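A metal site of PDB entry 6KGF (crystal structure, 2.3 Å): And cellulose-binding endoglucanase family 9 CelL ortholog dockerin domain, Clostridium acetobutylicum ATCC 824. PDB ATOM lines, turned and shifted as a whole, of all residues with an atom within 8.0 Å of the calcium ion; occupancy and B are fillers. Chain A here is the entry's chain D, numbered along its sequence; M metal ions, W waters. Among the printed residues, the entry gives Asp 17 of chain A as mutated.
Within 4 Å of the calcium ion: Asp 7, Asn 9, Asp 11, Val 13 and Asp 18.
The side-chain carboxylate of Asp 7 lies close to the backbone NH of Asp 10.
N of Gly 12 is in hydrogen-bond range of OD2 of Asp 7 (2.8 Å).
The backbone carbonyl oxygen of Asp 7 lies within hydrogen-bond range of the side-chain amide nitrogen of Asn 2, 2.8 Å away.
The side-chain carboxylate (OD2) of Asp 18 lies close to the backbone NH (N) of Asn 15, at 3.3 Å.
The side-chain carboxylate (OD1) of Asp 18 sits close to the backbone NH (N) of Leu 8.
The calcium ion is bound by OD1 of Asp 11 (2.3 Å), O of Val 13 (2.3 Å), OD1 of Asn 9 (2.4 Å), OD1 of Asp 7 (2.4 Å), OD2 of Asp 18 (2.4 Å), water W1 (2.5 Å) and OD1 of Asp 18 (2.6 Å).
The calcium ion has seven donor atoms within binding distance.
Water W1 lies within hydrogen-bond range of OD2 of Asp 11 (2.6 Å), OD1 of Asn 15 (2.6 Å) and ND2 of Asn 9 (2.8 Å).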
ATOM      1  N   ASN A   2      15.594  20.376  -4.618  1.00  0.00           N
ATOM      2  CA  ASN A   2      16.556  21.213  -3.908  1.00  0.00           C
ATOM      3  C   ASN A   2      16.666  22.536  -4.657  1.00  0.00           C
ATOM      4  O   ASN A   2      17.255  22.586  -5.749  1.00  0.00           O
ATOM      5  CB  ASN A   2      17.908  20.517  -3.805  1.00  0.00           C
ATOM      6  CG  ASN A   2      18.921  21.318  -3.011  1.00  0.00           C
ATOM      7  OD1 ASN A   2      18.688  22.479  -2.671  1.00  0.00           O
ATOM      8  ND2 ASN A   2      20.069  20.709  -2.733  1.00  0.00           N
ATOM      9  N   ILE A   4      17.984  25.501  -3.343  1.00  0.00           N
ATOM     10  CA  ILE A   4      18.902  26.412  -2.671  1.00  0.00           C
ATOM     11  C   ILE A   4      20.274  26.266  -3.335  1.00  0.00           C
ATOM     12  O   ILE A   4      20.855  25.171  -3.337  1.00  0.00           O
ATOM     13  CB  ILE A   4      18.981  26.125  -1.163  1.00  0.00           C
ATOM     14  CG1 ILE A   4      17.625  26.441  -0.522  1.00  0.00           C
ATOM     15  CG2 ILE A   4      20.103  26.939  -0.509  1.00  0.00           C
ATOM     16  CD1 ILE A   4      17.545  26.117   0.951  1.00  0.00           C
ATOM     17  N   LEU A   5      20.765  27.370  -3.883  1.00  0.00           N
ATOM     18  CA  LEU A   5      22.017  27.347  -4.650  1.00  0.00           C
ATOM     19  C   LEU A   5      23.197  27.111  -3.712  1.00  0.00           C
ATOM     20  O   LEU A   5      23.426  27.894  -2.781  1.00  0.00           O
ATOM     21  CB  LEU A   5      22.177  28.660  -5.405  1.00  0.00           C
ATOM     22  CG  LEU A   5      23.329  28.747  -6.408  1.00  0.00           C
ATOM     23  CD1 LEU A   5      23.114  27.786  -7.572  1.00  0.00           C
ATOM     24  CD2 LEU A   5      23.473  30.172  -6.908  1.00  0.00           C
ATOM     25  N   GLY A   6      23.941  26.043  -3.959  1.00  0.00           N
ATOM     26  CA  GLY A   6      25.096  25.700  -3.151  1.00  0.00           C
ATOM     27  C   GLY A   6      24.816  24.783  -1.988  1.00  0.00           C
ATOM     28  O   GLY A   6      25.743  24.460  -1.230  1.00  0.00           O
ATOM     29  N   ASP A   7      23.574  24.333  -1.816  1.00  0.00           N
ATOM     30  CA  ASP A   7      23.209  23.429  -0.728  1.00  0.00           C
ATOM     31  C   ASP A   7      23.479  21.997  -1.175  1.00  0.00           C
ATOM     32  O   ASP A   7      22.578  21.248  -1.591  1.00  0.00           O
ATOM     33  CB  ASP A   7      21.748  23.632  -0.328  1.00  0.00           C
ATOM     34  CG  ASP A   7      21.354  22.805   0.878  1.00  0.00           C
ATOM     35  OD1 ASP A   7      22.240  22.218   1.523  1.00  0.00           O
ATOM     36  OD2 ASP A   7      20.143  22.744   1.175  1.00  0.00           O
ATOM     37  N   LEU A   8      24.754  21.597  -1.086  1.00  0.00           N
ATOM     38  CA  LEU A   8      25.151  20.276  -1.581  1.00  0.00           C
ATOM     39  C   LEU A   8      24.590  19.151  -0.719  1.00  0.00           C
ATOM     40  O   LEU A   8      24.271  18.083  -1.252  1.00  0.00           O
ATOM     41  CB  LEU A   8      26.676  20.175  -1.642  1.00  0.00           C
ATOM     42  CG  LEU A   8      27.443  21.246  -2.433  1.00  0.00           C
ATOM     43  CD1 LEU A   8      28.817  20.717  -2.809  1.00  0.00           C
ATOM     44  CD2 LEU A   8      26.680  21.703  -3.669  1.00  0.00           C
ATOM     45  N   ASN A   9      24.469  19.356   0.593  1.00  0.00           N
ATOM     46  CA  ASN A   9      23.923  18.332   1.469  1.00  0.00           C
ATOM     47  C   ASN A   9      22.406  18.426   1.601  1.00  0.00           C
ATOM     48  O   ASN A   9      21.812  17.591   2.285  1.00  0.00           O
ATOM     49  CB  ASN A   9      24.567  18.422   2.854  1.00  0.00           C
ATOM     50  CG  ASN A   9      24.345  19.766   3.524  1.00  0.00           C
ATOM     51  OD1 ASN A   9      23.485  20.535   3.128  1.00  0.00           O
ATOM     52  ND2 ASN A   9      25.148  20.042   4.551  1.00  0.00           N
ATOM     53  N   ASP A  10      21.785  19.415   0.954  1.00  0.00           N
ATOM     54  CA  ASP A  10      20.319  19.539   0.933  1.00  0.00           C
ATOM     55  C   ASP A  10      19.745  19.597   2.347  1.00  0.00           C
ATOM     56  O   ASP A  10      18.807  18.879   2.682  1.00  0.00           O
ATOM     57  CB  ASP A  10      19.702  18.399   0.127  1.00  0.00           C
ATOM     58  CG  ASP A  10      18.236  18.644  -0.197  1.00  0.00           C
ATOM     59  OD1 ASP A  10      17.796  19.811  -0.126  1.00  0.00           O
ATOM     60  OD2 ASP A  10      17.529  17.668  -0.528  1.00  0.00           O
ATOM     61  N   ASP A  11      20.330  20.454   3.181  1.00  0.00           N
ATOM     62  CA  ASP A  11      19.859  20.649   4.546  1.00  0.00           C
ATOM     63  C   ASP A  11      19.163  21.999   4.749  1.00  0.00           C
ATOM     64  O   ASP A  11      18.739  22.298   5.868  1.00  0.00           O
ATOM     65  CB  ASP A  11      21.017  20.511   5.530  1.00  0.00           C
ATOM     66  CG  ASP A  11      22.048  21.614   5.392  1.00  0.00           C
ATOM     67  OD1 ASP A  11      21.940  22.407   4.426  1.00  0.00           O
ATOM     68  OD2 ASP A  11      22.968  21.691   6.237  1.00  0.00           O
ATOM     69  N   GLY A  12      19.043  22.816   3.701  1.00  0.00           N
ATOM     70  CA  GLY A  12      18.322  24.059   3.776  1.00  0.00           C
ATOM     71  C   GLY A  12      19.184  25.302   3.912  1.00  0.00           C
ATOM     72  O   GLY A  12      18.672  26.405   3.707  1.00  0.00           O
ATOM     73  N   VAL A  13      20.461  25.152   4.239  1.00  0.00           N
ATOM     74  CA  VAL A  13      21.353  26.279   4.454  1.00  0.00           C
ATOM     75  C   VAL A  13      22.632  26.082   3.647  1.00  0.00           C
ATOM     76  O   VAL A  13      22.923  24.987   3.149  1.00  0.00           O
ATOM     77  CB  VAL A  13      21.687  26.477   5.949  1.00  0.00           C
ATOM     78  CG1 VAL A  13      20.462  26.992   6.708  1.00  0.00           C
ATOM     79  CG2 VAL A  13      22.175  25.179   6.561  1.00  0.00           C
ATOM     80  N   VAL A  14      23.386  27.169   3.503  1.00  0.00           N
ATOM     81  CA  VAL A  14      24.638  27.190   2.762  1.00  0.00           C
ATOM     82  C   VAL A  14      25.720  27.648   3.717  1.00  0.00           C
ATOM     83  O   VAL A  14      25.773  28.830   4.090  1.00  0.00           O
ATOM     84  CB  VAL A  14      24.559  28.103   1.533  1.00  0.00           C
ATOM     85  CG1 VAL A  14      25.865  28.066   0.751  1.00  0.00           C
ATOM     86  CG2 VAL A  14      23.386  27.712   0.645  1.00  0.00           C
ATOM     87  N   ASN A  15      26.598  26.718   4.110  1.00  0.00           N
ATOM     88  CA  ASN A  15      27.625  27.018   5.100  1.00  0.00           C
ATOM     89  C   ASN A  15      28.865  26.182   4.774  1.00  0.00           C
ATOM     90  O   ASN A  15      28.992  25.645   3.675  1.00  0.00           O
ATOM     91  CB  ASN A  15      27.081  26.757   6.517  1.00  0.00           C
ATOM     92  CG  ASN A  15      26.582  25.333   6.701  1.00  0.00           C
ATOM     93  OD1 ASN A  15      26.910  24.437   5.924  1.00  0.00           O
ATOM     94  ND2 ASN A  15      25.784  25.123   7.738  1.00  0.00           N
ATOM     95  N   GLY A  16      29.777  26.069   5.746  1.00  0.00           N
ATOM     96  CA  GLY A  16      31.027  25.369   5.539  1.00  0.00           C
ATOM     97  C   GLY A  16      30.876  23.875   5.313  1.00  0.00           C
ATOM     98  O   GLY A  16      31.774  23.258   4.732  1.00  0.00           O
ATOM     99  N   ASP A  17      29.768  23.279   5.756  1.00  0.00           N
ATOM    100  CA  ASP A  17      29.555  21.863   5.494  1.00  0.00           C
ATOM    101  C   ASP A  17      29.397  21.597   4.001  1.00  0.00           C
ATOM    102  O   ASP A  17      29.835  20.551   3.513  1.00  0.00           O
ATOM    103  CB  ASP A  17      28.317  21.367   6.254  1.00  0.00           C
ATOM    104  CG  ASP A  17      28.490  21.459   7.751  1.00  0.00           C
ATOM    105  OD1 ASP A  17      29.642  21.486   8.230  1.00  0.00           O
ATOM    106  OD2 ASP A  17      27.467  21.503   8.472  1.00  0.00           O
ATOM    107  N   ASP A  18      28.778  22.524   3.278  1.00  0.00           N
ATOM    108  CA  ASP A  18      28.706  22.401   1.824  1.00  0.00           C
ATOM    109  C   ASP A  18      30.072  22.651   1.176  1.00  0.00           C
ATOM    110  O   ASP A  18      30.407  22.016   0.172  1.00  0.00           O
ATOM    111  CB  ASP A  18      27.666  23.366   1.266  1.00  0.00           C
ATOM    112  CG  ASP A  18      26.283  23.131   1.860  1.00  0.00           C
ATOM    113  OD1 ASP A  18      25.789  21.984   1.769  1.00  0.00           O
ATOM    114  OD2 ASP A  18      25.708  24.077   2.434  1.00  0.00           O
ATOM    115  N   ILE A  19      30.868  23.542   1.760  1.00  0.00           N
ATOM    116  CA  ILE A  19      32.231  23.756   1.281  1.00  0.00           C
ATOM    117  C   ILE A  19      33.035  22.478   1.430  1.00  0.00           C
ATOM    118  O   ILE A  19      33.826  22.107   0.548  1.00  0.00           O
ATOM    119  CB  ILE A  19      32.877  24.938   2.016  1.00  0.00           C
ATOM    120  CG1 ILE A  19      32.183  26.253   1.615  1.00  0.00           C
ATOM    121  CG2 ILE A  19      34.369  25.009   1.731  1.00  0.00           C
ATOM    122  CD1 ILE A  19      32.558  27.446   2.482  1.00  0.00           C
ATOM    123  N   MET A  21      31.990  19.378   1.351  1.00  0.00           N
ATOM    124  CA  MET A  21      31.587  18.427   0.324  1.00  0.00           C
ATOM    125  C   MET A  21      32.188  18.790  -1.033  1.00  0.00           C
ATOM    126  O   MET A  21      32.741  17.936  -1.732  1.00  0.00           O
ATOM    127  CB  MET A  21      30.065  18.362   0.242  1.00  0.00           C
ATOM    128  CG  MET A  21      29.413  17.599   1.383  1.00  0.00           C
ATOM    129  SD  MET A  21      27.670  17.210   1.067  1.00  0.00           S
ATOM    130  CE  MET A  21      27.346  16.068   2.408  1.00  0.00           C
ATOM    131  N   LEU A  55      30.940  29.118  -4.248  1.00  0.00           N
ATOM    132  CA  LEU A  55      30.335  28.655  -3.000  1.00  0.00           C
ATOM    133  C   LEU A  55      30.938  29.375  -1.795  1.00  0.00           C
ATOM    134  O   LEU A  55      30.220  29.770  -0.876  1.00  0.00           O
ATOM    135  CB  LEU A  55      30.502  27.144  -2.857  1.00  0.00           C
ATOM    136  CG  LEU A  55      29.896  26.494  -1.618  1.00  0.00           C
ATOM    137  CD1 LEU A  55      28.409  26.773  -1.523  1.00  0.00           C
ATOM    138  CD2 LEU A  55      30.166  25.002  -1.621  1.00  0.00           C
HETATM  139 CA    CA M   1      23.803  22.875   3.185  1.00  0.00          CA
HETATM  140  O   HOH W   1      25.087  22.736   5.269  1.00  0.00           O
